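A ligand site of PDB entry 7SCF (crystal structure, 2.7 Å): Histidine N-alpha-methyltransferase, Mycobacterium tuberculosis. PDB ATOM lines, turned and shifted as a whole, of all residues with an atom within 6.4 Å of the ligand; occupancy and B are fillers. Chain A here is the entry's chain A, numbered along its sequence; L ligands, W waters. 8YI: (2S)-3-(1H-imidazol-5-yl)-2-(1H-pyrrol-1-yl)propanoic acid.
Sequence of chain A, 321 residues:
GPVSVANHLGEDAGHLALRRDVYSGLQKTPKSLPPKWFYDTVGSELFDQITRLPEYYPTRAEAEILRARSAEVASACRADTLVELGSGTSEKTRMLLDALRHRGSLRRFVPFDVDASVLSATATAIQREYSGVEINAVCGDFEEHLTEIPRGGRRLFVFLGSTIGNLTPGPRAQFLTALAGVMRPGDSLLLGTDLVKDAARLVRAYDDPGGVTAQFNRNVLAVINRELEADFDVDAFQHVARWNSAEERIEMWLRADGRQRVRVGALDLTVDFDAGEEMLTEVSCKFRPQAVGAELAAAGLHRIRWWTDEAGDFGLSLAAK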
ATOM      1  N   PHE A  38     -14.502 -16.987  -0.032  1.00  0.00           N
ATOM      2  CA  PHE A  38     -15.282 -15.807   0.335  1.00  0.00           C
ATOM      3  C   PHE A  38     -16.350 -15.461  -0.705  1.00  0.00           C
ATOM      4  O   PHE A  38     -17.415 -14.928  -0.351  1.00  0.00           O
ATOM      5  CB  PHE A  38     -14.339 -14.608   0.504  1.00  0.00           C
ATOM      6  CG  PHE A  38     -13.524 -14.610   1.783  1.00  0.00           C
ATOM      7  CD1 PHE A  38     -14.099 -14.885   3.001  1.00  0.00           C
ATOM      8  CD2 PHE A  38     -12.181 -14.280   1.746  1.00  0.00           C
ATOM      9  CE1 PHE A  38     -13.348 -14.887   4.171  1.00  0.00           C
ATOM     10  CE2 PHE A  38     -11.410 -14.278   2.903  1.00  0.00           C
ATOM     11  CZ  PHE A  38     -12.008 -14.574   4.116  1.00  0.00           C
ATOM     12  N   TYR A  39     -16.098 -15.749  -1.981  1.00  0.00           N
ATOM     13  CA  TYR A  39     -16.812 -15.107  -3.083  1.00  0.00           C
ATOM     14  C   TYR A  39     -17.878 -16.024  -3.692  1.00  0.00           C
ATOM     15  O   TYR A  39     -17.873 -16.318  -4.879  1.00  0.00           O
ATOM     16  CB  TYR A  39     -15.809 -14.641  -4.135  1.00  0.00           C
ATOM     17  CG  TYR A  39     -14.739 -13.741  -3.555  1.00  0.00           C
ATOM     18  CD1 TYR A  39     -14.944 -12.368  -3.403  1.00  0.00           C
ATOM     19  CD2 TYR A  39     -13.521 -14.265  -3.128  1.00  0.00           C
ATOM     20  CE1 TYR A  39     -13.971 -11.561  -2.845  1.00  0.00           C
ATOM     21  CE2 TYR A  39     -12.551 -13.451  -2.588  1.00  0.00           C
ATOM     22  CZ  TYR A  39     -12.776 -12.111  -2.447  1.00  0.00           C
ATOM     23  OH  TYR A  39     -11.801 -11.312  -1.904  1.00  0.00           O
ATOM     24  N   PHE A  47     -18.371  -7.970  -0.756  1.00  0.00           N
ATOM     25  CA  PHE A  47     -17.173  -7.342  -1.278  1.00  0.00           C
ATOM     26  C   PHE A  47     -17.516  -6.092  -2.069  1.00  0.00           C
ATOM     27  O   PHE A  47     -16.707  -5.154  -2.153  1.00  0.00           O
ATOM     28  CB  PHE A  47     -16.371  -8.321  -2.126  1.00  0.00           C
ATOM     29  CG  PHE A  47     -15.092  -7.732  -2.637  1.00  0.00           C
ATOM     30  CD1 PHE A  47     -13.982  -7.680  -1.832  1.00  0.00           C
ATOM     31  CD2 PHE A  47     -15.036  -7.138  -3.884  1.00  0.00           C
ATOM     32  CE1 PHE A  47     -12.818  -7.093  -2.277  1.00  0.00           C
ATOM     33  CE2 PHE A  47     -13.892  -6.560  -4.340  1.00  0.00           C
ATOM     34  CZ  PHE A  47     -12.781  -6.533  -3.535  1.00  0.00           C
ATOM     35  N   ILE A  50     -17.534  -3.413   0.551  1.00  0.00           N
ATOM     36  CA  ILE A  50     -16.225  -3.058   1.061  1.00  0.00           C
ATOM     37  C   ILE A  50     -15.579  -2.016   0.158  1.00  0.00           C
ATOM     38  O   ILE A  50     -14.996  -1.035   0.644  1.00  0.00           O
ATOM     39  CB  ILE A  50     -15.345  -4.312   1.196  1.00  0.00           C
ATOM     40  CG1 ILE A  50     -16.043  -5.330   2.118  1.00  0.00           C
ATOM     41  CG2 ILE A  50     -14.001  -3.943   1.749  1.00  0.00           C
ATOM     42  CD1 ILE A  50     -15.145  -6.476   2.594  1.00  0.00           C
ATOM     43  N   TYR A  56     -11.789   1.771   3.068  1.00  0.00           N
ATOM     44  CA  TYR A  56     -11.181   0.862   2.088  1.00  0.00           C
ATOM     45  C   TYR A  56     -10.785   1.645   0.835  1.00  0.00           C
ATOM     46  O   TYR A  56     -11.533   1.736  -0.132  1.00  0.00           O
ATOM     47  CB  TYR A  56     -12.128  -0.300   1.771  1.00  0.00           C
ATOM     48  CG  TYR A  56     -11.474  -1.368   0.946  1.00  0.00           C
ATOM     49  CD1 TYR A  56     -10.692  -2.352   1.535  1.00  0.00           C
ATOM     50  CD2 TYR A  56     -11.618  -1.380  -0.445  1.00  0.00           C
ATOM     51  CE1 TYR A  56     -10.078  -3.319   0.761  1.00  0.00           C
ATOM     52  CE2 TYR A  56     -11.007  -2.339  -1.238  1.00  0.00           C
ATOM     53  CZ  TYR A  56     -10.239  -3.298  -0.624  1.00  0.00           C
ATOM     54  OH  TYR A  56      -9.628  -4.253  -1.392  1.00  0.00           O
ATOM     55  N   PRO A  58      -8.244   0.926  -1.481  1.00  0.00           N
ATOM     56  CA  PRO A  58      -7.587   0.354  -2.668  1.00  0.00           C
ATOM     57  C   PRO A  58      -8.395   0.426  -3.952  1.00  0.00           C
ATOM     58  O   PRO A  58      -7.815   0.752  -5.005  1.00  0.00           O
ATOM     59  CB  PRO A  58      -7.326  -1.102  -2.248  1.00  0.00           C
ATOM     60  CG  PRO A  58      -7.217  -1.020  -0.787  1.00  0.00           C
ATOM     61  CD  PRO A  58      -8.291  -0.074  -0.398  1.00  0.00           C
ATOM     62  N   LEU A 160      -5.534  -6.698 -11.624  1.00  0.00           N
ATOM     63  CA  LEU A 160      -5.607  -5.473 -10.831  1.00  0.00           C
ATOM     64  C   LEU A 160      -6.009  -5.763  -9.388  1.00  0.00           C
ATOM     65  O   LEU A 160      -6.162  -6.921  -8.971  1.00  0.00           O
ATOM     66  CB  LEU A 160      -6.603  -4.505 -11.475  1.00  0.00           C
ATOM     67  CG  LEU A 160      -6.334  -4.339 -12.968  1.00  0.00           C
ATOM     68  CD1 LEU A 160      -7.379  -3.471 -13.623  1.00  0.00           C
ATOM     69  CD2 LEU A 160      -4.963  -3.757 -13.168  1.00  0.00           C
ATOM     70  N   GLY A 161      -6.178  -4.680  -8.616  1.00  0.00           N
ATOM     71  CA  GLY A 161      -6.785  -4.729  -7.295  1.00  0.00           C
ATOM     72  C   GLY A 161      -5.921  -5.310  -6.207  1.00  0.00           C
ATOM     73  O   GLY A 161      -6.417  -5.522  -5.099  1.00  0.00           O
ATOM     74  N   SER A 162      -4.645  -5.570  -6.484  1.00  0.00           N
ATOM     75  CA  SER A 162      -3.736  -6.262  -5.573  1.00  0.00           C
ATOM     76  C   SER A 162      -4.193  -7.693  -5.293  1.00  0.00           C
ATOM     77  O   SER A 162      -3.896  -8.250  -4.229  1.00  0.00           O
ATOM     78  CB  SER A 162      -3.557  -5.495  -4.251  1.00  0.00           C
ATOM     79  OG  SER A 162      -2.364  -5.869  -3.611  1.00  0.00           O
ATOM     80  N   THR A 163      -4.942  -8.287  -6.244  1.00  0.00           N
ATOM     81  CA  THR A 163      -5.287  -9.697  -6.152  1.00  0.00           C
ATOM     82  C   THR A 163      -4.042 -10.555  -5.928  1.00  0.00           C
ATOM     83  O   THR A 163      -4.032 -11.471  -5.097  1.00  0.00           O
ATOM     84  CB  THR A 163      -6.025 -10.170  -7.429  1.00  0.00           C
ATOM     85  OG1 THR A 163      -6.981  -9.176  -7.816  1.00  0.00           O
ATOM     86  CG2 THR A 163      -6.763 -11.479  -7.176  1.00  0.00           C
ATOM     87  N   ILE A 164      -2.967 -10.257  -6.657  1.00  0.00           N
ATOM     88  CA  ILE A 164      -1.724 -10.980  -6.475  1.00  0.00           C
ATOM     89  C   ILE A 164      -1.247 -10.888  -5.035  1.00  0.00           C
ATOM     90  O   ILE A 164      -0.467 -11.751  -4.593  1.00  0.00           O
ATOM     91  CB  ILE A 164      -0.673 -10.446  -7.451  1.00  0.00           C
ATOM     92  CG1 ILE A 164       0.364 -11.530  -7.716  1.00  0.00           C
ATOM     93  CG2 ILE A 164      -0.042  -9.151  -6.907  1.00  0.00           C
ATOM     94  CD1 ILE A 164       1.562 -11.045  -8.465  1.00  0.00           C
ATOM     95  N   GLY A 165      -1.692  -9.871  -4.272  1.00  0.00           N
ATOM     96  CA  GLY A 165      -1.378  -9.784  -2.859  1.00  0.00           C
ATOM     97  C   GLY A 165      -1.973 -10.929  -2.065  1.00  0.00           C
ATOM     98  O   GLY A 165      -1.480 -11.246  -0.981  1.00  0.00           O
ATOM     99  N   ASN A 166      -3.003 -11.565  -2.606  1.00  0.00           N
ATOM    100  CA  ASN A 166      -3.551 -12.760  -1.963  1.00  0.00           C
ATOM    101  C   ASN A 166      -2.606 -13.941  -2.020  1.00  0.00           C
ATOM    102  O   ASN A 166      -2.910 -14.978  -1.412  1.00  0.00           O
ATOM    103  CB  ASN A 166      -4.888 -13.113  -2.611  1.00  0.00           C
ATOM    104  CG  ASN A 166      -6.063 -12.592  -1.833  1.00  0.00           C
ATOM    105  OD1 ASN A 166      -5.897 -11.981  -0.786  1.00  0.00           O
ATOM    106  ND2 ASN A 166      -7.254 -12.809  -2.350  1.00  0.00           N
ATOM    107  N   ASP A 194      -1.216  -3.015  -3.823  1.00  0.00           N
ATOM    108  CA  ASP A 194      -1.315  -2.112  -2.688  1.00  0.00           C
ATOM    109  C   ASP A 194       0.045  -2.018  -1.979  1.00  0.00           C
ATOM    110  O   ASP A 194       0.740  -3.024  -1.802  1.00  0.00           O
ATOM    111  CB  ASP A 194      -2.391  -2.573  -1.709  1.00  0.00           C
ATOM    112  CG  ASP A 194      -2.934  -1.431  -0.862  1.00  0.00           C
ATOM    113  OD1 ASP A 194      -2.630  -0.268  -1.195  1.00  0.00           O
ATOM    114  OD2 ASP A 194      -3.663  -1.682   0.108  1.00  0.00           O
ATOM    115  N   ALA A 205      -8.590  -0.397   7.262  1.00  0.00           N
ATOM    116  CA  ALA A 205      -9.096  -0.811   5.945  1.00  0.00           C
ATOM    117  C   ALA A 205      -9.667  -2.229   5.943  1.00  0.00           C
ATOM    118  O   ALA A 205     -10.426  -2.566   5.026  1.00  0.00           O
ATOM    119  CB  ALA A 205      -8.002  -0.706   4.887  1.00  0.00           C
ATOM    120  N   TYR A 206      -9.304  -3.068   6.906  1.00  0.00           N
ATOM    121  CA  TYR A 206      -9.733  -4.457   6.934  1.00  0.00           C
ATOM    122  C   TYR A 206     -10.553  -4.755   8.177  1.00  0.00           C
ATOM    123  O   TYR A 206     -10.751  -5.923   8.521  1.00  0.00           O
ATOM    124  CB  TYR A 206      -8.542  -5.403   6.821  1.00  0.00           C
ATOM    125  CG  TYR A 206      -7.929  -5.380   5.422  1.00  0.00           C
ATOM    126  CD1 TYR A 206      -6.927  -4.473   5.089  1.00  0.00           C
ATOM    127  CD2 TYR A 206      -8.374  -6.244   4.430  1.00  0.00           C
ATOM    128  CE1 TYR A 206      -6.387  -4.438   3.820  1.00  0.00           C
ATOM    129  CE2 TYR A 206      -7.837  -6.225   3.143  1.00  0.00           C
ATOM    130  CZ  TYR A 206      -6.844  -5.310   2.838  1.00  0.00           C
ATOM    131  OH  TYR A 206      -6.295  -5.278   1.565  1.00  0.00           O
ATOM    132  N   THR A 213     -16.655  -5.903   6.739  1.00  0.00           N
ATOM    133  CA  THR A 213     -15.555  -6.833   6.550  1.00  0.00           C
ATOM    134  C   THR A 213     -15.675  -8.018   7.479  1.00  0.00           C
ATOM    135  O   THR A 213     -15.301  -9.144   7.113  1.00  0.00           O
ATOM    136  CB  THR A 213     -14.236  -6.119   6.815  1.00  0.00           C
ATOM    137  OG1 THR A 213     -14.149  -4.953   6.005  1.00  0.00           O
ATOM    138  CG2 THR A 213     -13.062  -7.036   6.530  1.00  0.00           C
ATOM    139  N   PHE A 216     -17.995 -10.381   5.937  1.00  0.00           N
ATOM    140  CA  PHE A 216     -17.299 -10.952   4.787  1.00  0.00           C
ATOM    141  C   PHE A 216     -16.414 -12.110   5.215  1.00  0.00           C
ATOM    142  O   PHE A 216     -16.423 -13.175   4.595  1.00  0.00           O
ATOM    143  CB  PHE A 216     -16.493  -9.844   4.103  1.00  0.00           C
ATOM    144  CG  PHE A 216     -15.640 -10.324   2.951  1.00  0.00           C
ATOM    145  CD1 PHE A 216     -16.181 -10.448   1.686  1.00  0.00           C
ATOM    146  CD2 PHE A 216     -14.298 -10.587   3.124  1.00  0.00           C
ATOM    147  CE1 PHE A 216     -15.395 -10.876   0.603  1.00  0.00           C
ATOM    148  CE2 PHE A 216     -13.504 -11.014   2.060  1.00  0.00           C
ATOM    149  CZ  PHE A 216     -14.057 -11.167   0.797  1.00  0.00           C
ATOM    150  N   MET A 252      -6.170 -11.822   7.828  1.00  0.00           N
ATOM    151  CA  MET A 252      -7.541 -11.936   8.327  1.00  0.00           C
ATOM    152  C   MET A 252      -7.679 -13.272   9.051  1.00  0.00           C
ATOM    153  O   MET A 252      -7.507 -14.323   8.436  1.00  0.00           O
ATOM    154  CB  MET A 252      -8.573 -11.844   7.194  1.00  0.00           C
ATOM    155  CG  MET A 252      -8.763 -10.442   6.626  1.00  0.00           C
ATOM    156  SD  MET A 252     -10.495 -10.004   6.382  1.00  0.00           S
ATOM    157  CE  MET A 252     -10.984 -11.176   5.123  1.00  0.00           C
ATOM    158  N   GLU A 282      -7.236 -15.202   5.268  1.00  0.00           N
ATOM    159  CA  GLU A 282      -6.688 -14.404   4.181  1.00  0.00           C
ATOM    160  C   GLU A 282      -5.354 -13.805   4.592  1.00  0.00           C
ATOM    161  O   GLU A 282      -5.131 -13.480   5.760  1.00  0.00           O
ATOM    162  CB  GLU A 282      -7.657 -13.284   3.763  1.00  0.00           C
ATOM    163  CG  GLU A 282      -7.204 -12.466   2.558  1.00  0.00           C
ATOM    164  CD  GLU A 282      -8.207 -11.346   2.201  1.00  0.00           C
ATOM    165  OE1 GLU A 282      -8.598 -10.603   3.124  1.00  0.00           O
ATOM    166  OE2 GLU A 282      -8.587 -11.227   1.011  1.00  0.00           O
ATOM    167  N   VAL A 283      -4.459 -13.672   3.617  1.00  0.00           N
ATOM    168  CA  VAL A 283      -3.353 -12.726   3.723  1.00  0.00           C
ATOM    169  C   VAL A 283      -3.518 -11.721   2.595  1.00  0.00           C
ATOM    170  O   VAL A 283      -4.064 -12.025   1.530  1.00  0.00           O
ATOM    171  CB  VAL A 283      -1.957 -13.379   3.675  1.00  0.00           C
ATOM    172  CG1 VAL A 283      -1.884 -14.528   4.670  1.00  0.00           C
ATOM    173  CG2 VAL A 283      -1.611 -13.834   2.265  1.00  0.00           C
ATOM    174  N   SER A 284      -3.084 -10.507   2.844  1.00  0.00           N
ATOM    175  CA  SER A 284      -3.247  -9.417   1.895  1.00  0.00           C
ATOM    176  C   SER A 284      -1.896  -8.681   1.887  1.00  0.00           C
ATOM    177  O   SER A 284      -1.691  -7.659   2.551  1.00  0.00           O
ATOM    178  CB  SER A 284      -4.455  -8.540   2.258  1.00  0.00           C
ATOM    179  OG  SER A 284      -4.607  -7.399   1.429  1.00  0.00           O
ATOM    180  N   LYS A 286       1.246  -6.514   1.256  1.00  0.00           N
ATOM    181  CA  LYS A 286       1.488  -5.158   0.808  1.00  0.00           C
ATOM    182  C   LYS A 286       2.904  -5.051   0.252  1.00  0.00           C
ATOM    183  O   LYS A 286       3.799  -5.798   0.646  1.00  0.00           O
ATOM    184  CB  LYS A 286       1.284  -4.144   1.932  1.00  0.00           C
ATOM    185  CG  LYS A 286      -0.096  -4.228   2.612  1.00  0.00           C
ATOM    186  CD  LYS A 286      -1.219  -3.836   1.680  1.00  0.00           C
ATOM    187  CE  LYS A 286      -2.484  -4.604   2.011  1.00  0.00           C
ATOM    188  NZ  LYS A 286      -3.553  -4.339   1.003  1.00  0.00           N
HETATM  189  C10 8YI L   1     -10.451  -8.191   1.032  1.00  0.00           C
HETATM  190  N12 8YI L   1     -11.269  -6.734   2.397  1.00  0.00           N
HETATM  191  C13 8YI L   1     -10.991  -7.849   3.070  1.00  0.00           C
HETATM  192  C02 8YI L   1      -8.109  -7.124  -0.448  1.00  0.00           C
HETATM  193  C03 8YI L   1      -9.316  -7.764  -1.144  1.00  0.00           C
HETATM  194  C05 8YI L   1      -8.601  -9.663  -2.591  1.00  0.00           C
HETATM  195  C06 8YI L   1      -8.229  -9.801  -3.914  1.00  0.00           C
HETATM  196  C07 8YI L   1      -8.298  -8.583  -4.494  1.00  0.00           C
HETATM  197  C08 8YI L   1      -8.703  -7.685  -3.547  1.00  0.00           C
HETATM  198  C09 8YI L   1      -9.938  -8.838  -0.260  1.00  0.00           C
HETATM  199  C11 8YI L   1     -10.929  -6.924   1.146  1.00  0.00           C
HETATM  200  N04 8YI L   1      -8.887  -8.353  -2.395  1.00  0.00           N
HETATM  201  N14 8YI L   1     -10.493  -8.748   2.215  1.00  0.00           N
HETATM  202  O01 8YI L   1      -8.249  -6.019   0.129  1.00  0.00           O
HETATM  203  O15 8YI L   1      -6.976  -7.682  -0.473  1.00  0.00           O
HETATM  204  O   HOH W   1      -4.337  -8.426  -1.537  1.00  0.00           O
HETATM  205  O   HOH W   2     -12.281  -5.108   4.181  1.00  0.00           O
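O01 of the ligand sits at hydrogen-bond distance from OH of Tyr 206 (2.5 Å).
OG of Ser 284 is in hydrogen-bond range of O15 of the ligand, 3.1 Å away.
The side-chain carboxylate (OE1) of Glu 282 is in hydrogen-bond range of a nitrogen (N14) of the ligand.
An oxygen (O01) of the ligand is in hydrogen-bond range of the side-chain hydroxyl (OH) of Tyr 56 (2.7 Å).
The side-chain amide oxygen of Asn 166 lies close to the side-chain carboxylate of Glu 282 (3.3 Å).
The side-chain hydroxyl of Ser 284 is in hydrogen-bond range of the side-chain amino group of Lys 286, at 3.3 Å.
The backbone NH of Met 252 sits at hydrogen-bond distance from the backbone carbonyl oxygen of Glu 282.
OG of Ser 284 lies within hydrogen-bond range of OH of Tyr 206 (2.7 Å).
The side-chain amide oxygen of Asn 166 lies close to the backbone carbonyl oxygen of Val 283 (3.0 Å).
O of Leu 160 is in hydrogen-bond range of OG1 of Thr 163 (2.7 Å).
The side-chain amino group of Lys 286 sits at hydrogen-bond distance from the side-chain hydroxyl of Tyr 206 (3.0 Å).
Tyr 39 touches the ligand.
CE1 of Phe 47 touches C03 of the ligand (3.7 Å).
CD1 of Ile 50 touches N12 of the ligand (3.9 Å).
Gly 161 touches the ligand.
Thr 163 touches the ligand (CA to C07, 3.6 Å).
Asn 166 touches the ligand (ND2 to C05, 3.4 Å).
Phe 216 touches the ligand.
Met 252 touches the ligand (CE to N14, 3.8 Å).
Of the 23 residues printed, 12 come within 4 Å of the ligand.
Along chain A the residues within 4 Å of the ligand span positions 39 to 284.
Water W2 lies within hydrogen-bond range of OG1 of Thr 213, N12 of the ligand and O of Ala 205.
Water W1 lies within hydrogen-bond range of O of Ser 162, O15 of the ligand and OG of Ser 284.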
